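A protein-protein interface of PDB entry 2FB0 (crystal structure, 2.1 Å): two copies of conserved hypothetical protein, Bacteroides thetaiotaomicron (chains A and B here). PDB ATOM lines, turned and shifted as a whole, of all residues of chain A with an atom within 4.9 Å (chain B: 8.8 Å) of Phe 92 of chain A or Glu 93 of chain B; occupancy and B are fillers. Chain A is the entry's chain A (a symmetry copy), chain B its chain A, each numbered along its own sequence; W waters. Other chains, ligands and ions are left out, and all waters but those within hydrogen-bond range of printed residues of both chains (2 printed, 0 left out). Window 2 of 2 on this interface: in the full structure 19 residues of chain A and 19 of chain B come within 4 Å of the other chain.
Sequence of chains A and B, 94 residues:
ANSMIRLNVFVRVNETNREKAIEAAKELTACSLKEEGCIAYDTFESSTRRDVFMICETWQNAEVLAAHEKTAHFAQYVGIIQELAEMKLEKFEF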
ATOM      1  N   MET A   4      11.807   4.221  26.040  1.00  0.00           N
ATOM      2  CA  MET A   4      11.351   5.211  27.013  1.00  0.00           C
ATOM      3  C   MET A   4      11.583   6.621  26.457  1.00  0.00           C
ATOM      4  O   MET A   4      12.426   6.828  25.580  1.00  0.00           O
ATOM      5  CB  MET A   4      12.055   5.057  28.362  1.00  0.00           C
ATOM      6  CG  MET A   4      11.526   3.901  29.222  1.00  0.00           C
ATOM      7  SD  MET A   4      12.513   3.861  30.865  1.00  0.00           S
ATOM      8  CE  MET A   4      14.196   3.283  30.164  1.00  0.00           C
ATOM      9  N   ILE A   5      10.811   7.577  26.958  1.00  0.00           N
ATOM     10  CA  ILE A   5      10.908   8.959  26.500  1.00  0.00           C
ATOM     11  C   ILE A   5      11.214   9.857  27.687  1.00  0.00           C
ATOM     12  O   ILE A   5      10.547   9.782  28.723  1.00  0.00           O
ATOM     13  CB  ILE A   5       9.601   9.425  25.807  1.00  0.00           C
ATOM     14  CG1 ILE A   5       9.399   8.676  24.485  1.00  0.00           C
ATOM     15  CG2 ILE A   5       9.606  10.944  25.569  1.00  0.00           C
ATOM     16  CD1 ILE A   5       8.018   8.860  23.882  1.00  0.00           C
ATOM     17  N   ARG A   6      12.229  10.694  27.524  1.00  0.00           N
ATOM     18  CA  ARG A   6      12.571  11.705  28.515  1.00  0.00           C
ATOM     19  C   ARG A   6      12.078  13.070  28.026  1.00  0.00           C
ATOM     20  O   ARG A   6      12.388  13.481  26.905  1.00  0.00           O
ATOM     21  CB  ARG A   6      14.092  11.730  28.757  1.00  0.00           C
ATOM     22  CG  ARG A   6      14.620  12.952  29.550  1.00  0.00           C
ATOM     23  CD  ARG A   6      14.040  13.069  30.979  1.00  0.00           C
ATOM     24  NE  ARG A   6      14.024  11.780  31.682  1.00  0.00           N
ATOM     25  CZ  ARG A   6      15.099  11.223  32.242  1.00  0.00           C
ATOM     26  NH1 ARG A   6      16.276  11.857  32.216  1.00  0.00           N
ATOM     27  NH2 ARG A   6      14.995  10.041  32.860  1.00  0.00           N
ATOM     28  N   ASN A   8      12.208  17.177  29.054  1.00  0.00           N
ATOM     29  CA  ASN A   8      12.661  18.311  29.836  1.00  0.00           C
ATOM     30  C   ASN A   8      11.811  19.517  29.430  1.00  0.00           C
ATOM     31  O   ASN A   8      11.901  19.994  28.295  1.00  0.00           O
ATOM     32  CB  ASN A   8      14.136  18.628  29.563  1.00  0.00           C
ATOM     33  CG  ASN A   8      15.107  17.523  30.039  1.00  0.00           C
ATOM     34  OD1 ASN A   8      14.736  16.595  30.785  1.00  0.00           O
ATOM     35  ND2 ASN A   8      16.348  17.626  29.601  1.00  0.00           N
ATOM     36  N   GLU A  90      11.081  19.860  25.513  1.00  0.00           N
ATOM     37  CA  GLU A  90      12.076  19.136  24.727  1.00  0.00           C
ATOM     38  C   GLU A  90      11.924  17.641  25.022  1.00  0.00           C
ATOM     39  O   GLU A  90      11.782  17.239  26.184  1.00  0.00           O
ATOM     40  CB  GLU A  90      13.499  19.618  25.031  1.00  0.00           C
ATOM     41  CG  GLU A  90      13.697  21.131  24.838  1.00  0.00           C
ATOM     42  CD  GLU A  90      15.151  21.564  24.872  1.00  0.00           C
ATOM     43  OE1 GLU A  90      15.915  21.148  25.771  1.00  0.00           O
ATOM     44  OE2 GLU A  90      15.535  22.345  23.983  1.00  0.00           O
ATOM     45  N   LYS A  91      11.943  16.844  23.958  1.00  0.00           N
ATOM     46  CA  LYS A  91      11.708  15.408  24.010  1.00  0.00           C
ATOM     47  C   LYS A  91      12.928  14.629  23.505  1.00  0.00           C
ATOM     48  O   LYS A  91      13.531  14.998  22.502  1.00  0.00           O
ATOM     49  CB  LYS A  91      10.469  15.064  23.169  1.00  0.00           C
ATOM     50  CG  LYS A  91      10.295  13.568  22.842  1.00  0.00           C
ATOM     51  CD  LYS A  91       8.813  13.193  22.642  1.00  0.00           C
ATOM     52  CE  LYS A  91       8.172  13.865  21.435  1.00  0.00           C
ATOM     53  NZ  LYS A  91       6.671  13.665  21.434  1.00  0.00           N
ATOM     54  N   PHE A  92      13.282  13.555  24.214  1.00  0.00           N
ATOM     55  CA  PHE A  92      14.423  12.700  23.856  1.00  0.00           C
ATOM     56  C   PHE A  92      14.028  11.230  24.046  1.00  0.00           C
ATOM     57  O   PHE A  92      13.221  10.906  24.914  1.00  0.00           O
ATOM     58  CB  PHE A  92      15.634  13.007  24.748  1.00  0.00           C
ATOM     59  CG  PHE A  92      16.022  14.464  24.783  1.00  0.00           C
ATOM     60  CD1 PHE A  92      15.488  15.318  25.748  1.00  0.00           C
ATOM     61  CD2 PHE A  92      16.933  14.979  23.854  1.00  0.00           C
ATOM     62  CE1 PHE A  92      15.848  16.675  25.787  1.00  0.00           C
ATOM     63  CE2 PHE A  92      17.290  16.336  23.884  1.00  0.00           C
ATOM     64  CZ  PHE A  92      16.743  17.177  24.857  1.00  0.00           C
ATOM     65  N   GLU A  93      14.582  10.353  23.219  1.00  0.00           N
ATOM     66  CA  GLU A  93      14.368   8.917  23.384  1.00  0.00           C
ATOM     67  C   GLU A  93      15.583   8.282  24.042  1.00  0.00           C
ATOM     68  O   GLU A  93      16.725   8.683  23.779  1.00  0.00           O
ATOM     69  CB  GLU A  93      14.107   8.232  22.041  1.00  0.00           C
ATOM     70  CG  GLU A  93      12.738   8.539  21.444  1.00  0.00           C
ATOM     71  CD  GLU A  93      12.334   7.570  20.343  1.00  0.00           C
ATOM     72  OE1 GLU A  93      12.982   6.504  20.194  1.00  0.00           O
ATOM     73  OE2 GLU A  93      11.353   7.872  19.625  1.00  0.00           O
ATOM     74  N   PHE A  94      15.325   7.306  24.907  1.00  0.00           N
ATOM     75  CA  PHE A  94      16.377   6.470  25.461  1.00  0.00           C
ATOM     76  C   PHE A  94      16.932   5.614  24.328  1.00  0.00           C
ATOM     77  O   PHE A  94      18.046   5.100  24.387  1.00  0.00           O
ATOM     78  CB  PHE A  94      15.825   5.580  26.582  1.00  0.00           C
ATOM     79  CG  PHE A  94      15.706   6.281  27.913  1.00  0.00           C
ATOM     80  CD1 PHE A  94      14.737   7.260  28.120  1.00  0.00           C
ATOM     81  CD2 PHE A  94      16.568   5.960  28.957  1.00  0.00           C
ATOM     82  CE1 PHE A  94      14.624   7.912  29.349  1.00  0.00           C
ATOM     83  CE2 PHE A  94      16.463   6.608  30.190  1.00  0.00           C
ATOM     84  CZ  PHE A  94      15.482   7.589  30.380  1.00  0.00           C
ATOM     85  OXT PHE A  94      16.263   5.437  23.313  1.00  0.00           O
ATOM     86  N   ALA B   1      26.194  12.491  16.563  1.00  0.00           N
ATOM     87  CA  ALA B   1      27.220  13.335  15.868  1.00  0.00           C
ATOM     88  C   ALA B   1      26.684  13.909  14.540  1.00  0.00           C
ATOM     89  O   ALA B   1      25.998  13.197  13.790  1.00  0.00           O
ATOM     90  CB  ALA B   1      28.499  12.531  15.637  1.00  0.00           C
ATOM     91  N   ASN B   2      26.937  15.192  14.256  1.00  0.00           N
ATOM     92  CA  ASN B   2      27.511  16.166  15.197  1.00  0.00           C
ATOM     93  C   ASN B   2      26.415  16.782  16.073  1.00  0.00           C
ATOM     94  O   ASN B   2      26.289  18.002  16.183  1.00  0.00           O
ATOM     95  CB  ASN B   2      28.230  17.277  14.424  1.00  0.00           C
ATOM     96  CG  ASN B   2      29.730  17.059  14.343  1.00  0.00           C
ATOM     97  OD1 ASN B   2      30.207  16.138  13.668  1.00  0.00           O
ATOM     98  ND2 ASN B   2      30.488  17.918  15.033  1.00  0.00           N
ATOM     99  N   SER B   3      25.619  15.918  16.683  1.00  0.00           N
ATOM    100  CA  SER B   3      24.416  16.326  17.383  1.00  0.00           C
ATOM    101  C   SER B   3      24.723  16.922  18.754  1.00  0.00           C
ATOM    102  O   SER B   3      25.716  16.565  19.376  1.00  0.00           O
ATOM    103  CB  SER B   3      23.493  15.119  17.524  1.00  0.00           C
ATOM    104  OG  SER B   3      22.153  15.542  17.702  1.00  0.00           O
ATOM    105  N   MET B   4      23.874  17.844  19.212  1.00  0.00           N
ATOM    106  CA  MET B   4      23.972  18.345  20.581  1.00  0.00           C
ATOM    107  C   MET B   4      23.674  17.207  21.566  1.00  0.00           C
ATOM    108  O   MET B   4      23.018  16.222  21.219  1.00  0.00           O
ATOM    109  CB  MET B   4      23.023  19.518  20.833  1.00  0.00           C
ATOM    110  CG  MET B   4      23.508  20.857  20.259  1.00  0.00           C
ATOM    111  SD  MET B   4      22.208  22.203  20.670  1.00  0.00           S
ATOM    112  CE  MET B   4      20.808  21.600  19.515  1.00  0.00           C
ATOM    113  N   ILE B   5      24.184  17.345  22.783  1.00  0.00           N
ATOM    114  CA  ILE B   5      23.999  16.326  23.810  1.00  0.00           C
ATOM    115  C   ILE B   5      23.328  16.954  25.020  1.00  0.00           C
ATOM    116  O   ILE B   5      23.762  18.001  25.510  1.00  0.00           O
ATOM    117  CB  ILE B   5      25.349  15.685  24.228  1.00  0.00           C
ATOM    118  CG1 ILE B   5      25.929  14.859  23.075  1.00  0.00           C
ATOM    119  CG2 ILE B   5      25.188  14.815  25.485  1.00  0.00           C
ATOM    120  CD1 ILE B   5      27.369  14.430  23.293  1.00  0.00           C
ATOM    121  N   ARG B   6      22.266  16.309  25.484  1.00  0.00           N
ATOM    122  CA  ARG B   6      21.586  16.707  26.708  1.00  0.00           C
ATOM    123  C   ARG B   6      21.982  15.748  27.835  1.00  0.00           C
ATOM    124  O   ARG B   6      21.865  14.529  27.686  1.00  0.00           O
ATOM    125  CB  ARG B   6      20.060  16.705  26.502  1.00  0.00           C
ATOM    126  CG  ARG B   6      19.213  16.812  27.795  1.00  0.00           C
ATOM    127  CD  ARG B   6      19.453  18.114  28.595  1.00  0.00           C
ATOM    128  NE  ARG B   6      19.493  19.299  27.731  1.00  0.00           N
ATOM    129  CZ  ARG B   6      18.409  19.893  27.228  1.00  0.00           C
ATOM    130  NH1 ARG B   6      17.190  19.436  27.531  1.00  0.00           N
ATOM    131  NH2 ARG B   6      18.538  20.969  26.445  1.00  0.00           N
ATOM    132  N   LEU B   7      22.449  16.301  28.953  1.00  0.00           N
ATOM    133  CA  LEU B   7      22.653  15.503  30.172  1.00  0.00           C
ATOM    134  C   LEU B   7      21.643  15.887  31.236  1.00  0.00           C
ATOM    135  O   LEU B   7      21.369  17.072  31.439  1.00  0.00           O
ATOM    136  CB  LEU B   7      24.074  15.661  30.739  1.00  0.00           C
ATOM    137  CG  LEU B   7      25.295  15.411  29.837  1.00  0.00           C
ATOM    138  CD1 LEU B   7      26.570  15.488  30.662  1.00  0.00           C
ATOM    139  CD2 LEU B   7      25.206  14.057  29.182  1.00  0.00           C
ATOM    140  N   ASN B   8      21.077  14.869  31.878  1.00  0.00           N
ATOM    141  CA  ASN B   8      20.317  15.014  33.104  1.00  0.00           C
ATOM    142  C   ASN B   8      21.062  14.246  34.198  1.00  0.00           C
ATOM    143  O   ASN B   8      21.153  13.016  34.150  1.00  0.00           O
ATOM    144  CB  ASN B   8      18.906  14.433  32.962  1.00  0.00           C
ATOM    145  CG  ASN B   8      18.015  15.203  31.960  1.00  0.00           C
ATOM    146  OD1 ASN B   8      18.340  16.320  31.511  1.00  0.00           O
ATOM    147  ND2 ASN B   8      16.894  14.599  31.611  1.00  0.00           N
ATOM    148  N   CYS B  56      21.135  19.944  34.759  1.00  0.00           N
ATOM    149  CA  CYS B  56      20.727  19.855  33.367  1.00  0.00           C
ATOM    150  C   CYS B  56      21.785  20.545  32.514  1.00  0.00           C
ATOM    151  O   CYS B  56      22.170  21.676  32.798  1.00  0.00           O
ATOM    152  CB  CYS B  56      19.371  20.535  33.168  1.00  0.00           C
ATOM    153  SG  CYS B  56      18.623  20.125  31.577  1.00  0.00           S
ATOM    154  N   GLU B  57      22.266  19.861  31.481  1.00  0.00           N
ATOM    155  CA  GLU B  57      23.351  20.391  30.669  1.00  0.00           C
ATOM    156  C   GLU B  57      23.037  20.192  29.210  1.00  0.00           C
ATOM    157  O   GLU B  57      22.405  19.216  28.846  1.00  0.00           O
ATOM    158  CB  GLU B  57      24.669  19.670  30.981  1.00  0.00           C
ATOM    159  CG  GLU B  57      24.899  19.488  32.465  1.00  0.00           C
ATOM    160  CD  GLU B  57      26.090  18.622  32.798  1.00  0.00           C
ATOM    161  OE1 GLU B  57      27.034  18.526  31.990  1.00  0.00           O
ATOM    162  OE2 GLU B  57      26.073  18.049  33.904  1.00  0.00           O
ATOM    163  N   THR B  58      23.507  21.116  28.375  1.00  0.00           N
ATOM    164  CA  THR B  58      23.506  20.901  26.939  1.00  0.00           C
ATOM    165  C   THR B  58      24.896  21.192  26.399  1.00  0.00           C
ATOM    166  O   THR B  58      25.466  22.258  26.655  1.00  0.00           O
ATOM    167  CB  THR B  58      22.473  21.787  26.229  1.00  0.00           C
ATOM    168  OG1 THR B  58      21.214  21.630  26.880  1.00  0.00           O
ATOM    169  CG2 THR B  58      22.342  21.410  24.739  1.00  0.00           C
ATOM    170  N   TRP B  59      25.425  20.229  25.653  1.00  0.00           N
ATOM    171  CA  TRP B  59      26.760  20.305  25.086  1.00  0.00           C
ATOM    172  C   TRP B  59      26.658  20.332  23.578  1.00  0.00           C
ATOM    173  O   TRP B  59      25.808  19.655  22.998  1.00  0.00           O
ATOM    174  CB  TRP B  59      27.640  19.144  25.584  1.00  0.00           C
ATOM    175  CG  TRP B  59      27.923  19.349  27.035  1.00  0.00           C
ATOM    176  CD1 TRP B  59      27.217  18.840  28.094  1.00  0.00           C
ATOM    177  CD2 TRP B  59      28.916  20.211  27.589  1.00  0.00           C
ATOM    178  NE1 TRP B  59      27.732  19.324  29.279  1.00  0.00           N
ATOM    179  CE2 TRP B  59      28.774  20.166  28.993  1.00  0.00           C
ATOM    180  CE3 TRP B  59      29.923  21.018  27.032  1.00  0.00           C
ATOM    181  CZ2 TRP B  59      29.609  20.884  29.850  1.00  0.00           C
ATOM    182  CZ3 TRP B  59      30.748  21.731  27.885  1.00  0.00           C
ATOM    183  CH2 TRP B  59      30.581  21.666  29.277  1.00  0.00           C
ATOM    184  N   ASN B  61      28.522  19.155  21.261  1.00  0.00           N
ATOM    185  CA  ASN B  61      28.806  17.858  20.672  1.00  0.00           C
ATOM    186  C   ASN B  61      29.592  16.994  21.655  1.00  0.00           C
ATOM    187  O   ASN B  61      29.948  17.443  22.766  1.00  0.00           O
ATOM    188  CB  ASN B  61      29.588  18.013  19.350  1.00  0.00           C
ATOM    189  CG  ASN B  61      30.839  18.853  19.508  1.00  0.00           C
ATOM    190  OD1 ASN B  61      31.728  18.515  20.289  1.00  0.00           O
ATOM    191  ND2 ASN B  61      30.914  19.963  18.772  1.00  0.00           N
ATOM    192  N   ALA B  62      29.858  15.763  21.234  1.00  0.00           N
ATOM    193  CA  ALA B  62      30.572  14.779  22.053  1.00  0.00           C
ATOM    194  C   ALA B  62      31.989  15.197  22.409  1.00  0.00           C
ATOM    195  O   ALA B  62      32.481  14.872  23.498  1.00  0.00           O
ATOM    196  CB  ALA B  62      30.571  13.400  21.364  1.00  0.00           C
ATOM    197  N   GLU B  90      22.559  10.706  33.094  1.00  0.00           N
ATOM    198  CA  GLU B  90      21.863  10.184  31.921  1.00  0.00           C
ATOM    199  C   GLU B  90      22.150  11.115  30.739  1.00  0.00           C
ATOM    200  O   GLU B  90      22.094  12.343  30.876  1.00  0.00           O
ATOM    201  CB  GLU B  90      20.356  10.052  32.168  1.00  0.00           C
ATOM    202  CG  GLU B  90      20.000   9.199  33.397  1.00  0.00           C
ATOM    203  CD  GLU B  90      18.527   8.844  33.486  1.00  0.00           C
ATOM    204  OE1 GLU B  90      17.652   9.721  33.311  1.00  0.00           O
ATOM    205  OE2 GLU B  90      18.239   7.661  33.743  1.00  0.00           O
ATOM    206  N   LYS B  91      22.468  10.509  29.599  1.00  0.00           N
ATOM    207  CA  LYS B  91      22.880  11.208  28.391  1.00  0.00           C
ATOM    208  C   LYS B  91      21.915  10.929  27.234  1.00  0.00           C
ATOM    209  O   LYS B  91      21.495   9.793  27.032  1.00  0.00           O
ATOM    210  CB  LYS B  91      24.305  10.776  28.013  1.00  0.00           C
ATOM    211  CG  LYS B  91      24.748  11.156  26.586  1.00  0.00           C
ATOM    212  CD  LYS B  91      26.275  11.341  26.488  1.00  0.00           C
ATOM    213  CE  LYS B  91      27.061  10.062  26.741  1.00  0.00           C
ATOM    214  NZ  LYS B  91      28.541  10.352  26.884  1.00  0.00           N
ATOM    215  N   PHE B  92      21.566  11.977  26.484  1.00  0.00           N
ATOM    216  CA  PHE B  92      20.656  11.872  25.335  1.00  0.00           C
ATOM    217  C   PHE B  92      21.197  12.732  24.186  1.00  0.00           C
ATOM    218  O   PHE B  92      21.836  13.756  24.417  1.00  0.00           O
ATOM    219  CB  PHE B  92      19.252  12.370  25.706  1.00  0.00           C
ATOM    220  CG  PHE B  92      18.671  11.718  26.936  1.00  0.00           C
ATOM    221  CD1 PHE B  92      18.865  12.281  28.197  1.00  0.00           C
ATOM    222  CD2 PHE B  92      17.918  10.543  26.828  1.00  0.00           C
ATOM    223  CE1 PHE B  92      18.322  11.680  29.345  1.00  0.00           C
ATOM    224  CE2 PHE B  92      17.381   9.934  27.973  1.00  0.00           C
ATOM    225  CZ  PHE B  92      17.588  10.512  29.229  1.00  0.00           C
ATOM    226  N   GLU B  93      20.958  12.299  22.954  1.00  0.00           N
ATOM    227  CA  GLU B  93      21.325  13.096  21.787  1.00  0.00           C
ATOM    228  C   GLU B  93      20.096  13.792  21.224  1.00  0.00           C
ATOM    229  O   GLU B  93      18.993  13.229  21.232  1.00  0.00           O
ATOM    230  CB  GLU B  93      21.958  12.231  20.695  1.00  0.00           C
ATOM    231  CG  GLU B  93      23.368  11.753  21.022  1.00  0.00           C
ATOM    232  CD  GLU B  93      24.126  11.247  19.805  1.00  0.00           C
ATOM    233  OE1 GLU B  93      23.676  11.486  18.656  1.00  0.00           O
ATOM    234  OE2 GLU B  93      25.188  10.610  19.996  1.00  0.00           O
ATOM    235  N   PHE B  94      20.293  15.021  20.756  1.00  0.00           N
ATOM    236  CA  PHE B  94      19.270  15.733  20.007  1.00  0.00           C
ATOM    237  C   PHE B  94      19.092  15.018  18.672  1.00  0.00           C
ATOM    238  O   PHE B  94      18.072  15.141  17.999  1.00  0.00           O
ATOM    239  CB  PHE B  94      19.685  17.192  19.780  1.00  0.00           C
ATOM    240  CG  PHE B  94      19.421  18.091  20.962  1.00  0.00           C
ATOM    241  CD1 PHE B  94      20.180  17.984  22.125  1.00  0.00           C
ATOM    242  CD2 PHE B  94      18.408  19.043  20.910  1.00  0.00           C
ATOM    243  CE1 PHE B  94      19.938  18.813  23.222  1.00  0.00           C
ATOM    244  CE2 PHE B  94      18.157  19.876  22.003  1.00  0.00           C
ATOM    245  CZ  PHE B  94      18.932  19.755  23.163  1.00  0.00           C
ATOM    246  OXT PHE B  94      19.981  14.280  18.252  1.00  0.00           O
HETATM  247  O   HOH W   1      19.277   9.836  22.786  1.00  0.00           O
HETATM  248  O   HOH W   2      16.579  11.497  21.316  1.00  0.00           O
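NH2 of Arg 6 of chain B lies within salt-bridge range of OE1 of Glu 90 of chain A, at 2.7 Å. The side-chain amide nitrogen (ND2) of Asn 8 of chain B lies within hydrogen-bond range of the side-chain amide oxygen (OD1) of Asn 8 of chain A (3.1 Å). The guanidinium group (NH1) of Arg 6 of chain B sits close to the side-chain amide nitrogen (ND2) of Asn 8 of chain A, 2.9 Å away. ND2 of Asn 8 of chain B lies close to NH1 of Arg 6 of chain A (2.9 Å). The guanidinium group (NH2) of Arg 6 of chain A lies within salt-bridge range of the side-chain carboxylate (OE1) of Glu 90 of chain B (2.7 Å).
N of Asn 8 of chain B lies within hydrogen-bond range of O of Glu 90 of chain B. The guanidinium group of Arg 6 of chain B is in hydrogen-bond range of the side-chain hydroxyl of Thr 58 of chain B (2.8 Å). OG of Ser 3 of chain B is in hydrogen-bond range of OXT of Phe 94 of chain B, at 2.6 Å. The backbone carbonyl oxygen (O) of Phe 92 of chain A sits at hydrogen-bond distance from the backbone NH (N) of Arg 6 of chain A (2.8 Å). O of Met 4 of chain A is in hydrogen-bond range of N of Phe 94 of chain A (3.0 Å). The side-chain carboxylate (OE1) of Glu 93 of chain B lies within hydrogen-bond range of the backbone NH (N) of Ala 1 of chain B, 3.4 Å away.
Arg 6 of chain A touches Phe 92 of chain B (NH1 to CZ, 3.5 Å). Asn 8 of chain A touches Cys 56 of chain B (ND2 to SG, 3.9 Å). CZ of Phe 92 of chain A touches NH1 of Arg 6 of chain B, 3.5 Å away. Phe 92 of chain B touches Phe 92 of chain A. Glu 93 of chain B touches Phe 92 of chain A. Phe 92 of chain A touches Phe 94 of chain B (CE2 to CE1, 3.7 Å). Glu 93 of chain A touches Phe 92 of chain B (O to CD2, 3.8 Å). Phe 94 of chain A touches Phe 92 of chain B (CE1 to CE2, 3.7 Å).
Phe 92 of chain A touches just these residues of chain B: Arg 6 (3.5 Å), Phe 92 (3.8 Å), Glu 93 (3.8 Å) and Phe 94 (3.7 Å). Glu 93 of chain B touches just one residue of chain A: Phe 92. Of the printed residues of chain A, Phe 94 of chain B touches Phe 92. Printed residues of chain A within 4 Å of Asn 8 of chain B: Arg 6 (2.9 Å) and Asn 8 (3.1 Å). Met 4 of chain B touches none of the printed residues of chain A.
Printed residues of chain B that touch a printed residue of chain A: Arg 6, Asn 8, Cys 56, Glu 90, Phe 92, Glu 93 and Phe 94. Hydrophobic or aromatic side chains of chain B within 4 Å of the printed part of chain A: Phe 92 and Phe 94. Of the 9 printed residues of chain A, 6 touch a printed residue of chain B. Hydrophobic or aromatic side chains of chain A within 4 Å of the printed part of chain B: Phe 92 and Phe 94. Among the printed residues, 13 pairs touch across the chains. Among the printed residues, Asp or Glu carboxylates within 4 Å of a Lys or Arg side-chain nitrogen of the other chain: Arg 6 of chain A with Glu 90 of chain B (2.7 Å) and Glu 90 of chain A with Arg 6 of chain B (2.7 Å).
Arg 6 of chain A touches Glu 90 of chain B, and with the chains exchanged Glu 90 of chain A touches Arg 6 of chain B. Arg 6 of chain A touches Phe 92 of chain B, and with the chains exchanged Phe 92 of chain A touches Arg 6 of chain B. Asn 8 of chain B touches its own counterpart, Asn 8 of chain A. Phe 92 of chain A touches Glu 93 of chain B, and with the chains exchanged Glu 93 of chain A touches Phe 92 of chain B.
Water W1 lies within hydrogen-bond range of the backbone carbonyl oxygen (O) of Glu 93 of chain A (3.0 Å) and the backbone NH (N) of Glu 93 of chain B (3.0 Å). Water W2 bridges O of Glu 93 of chain B and N of Glu 93 of chain A.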
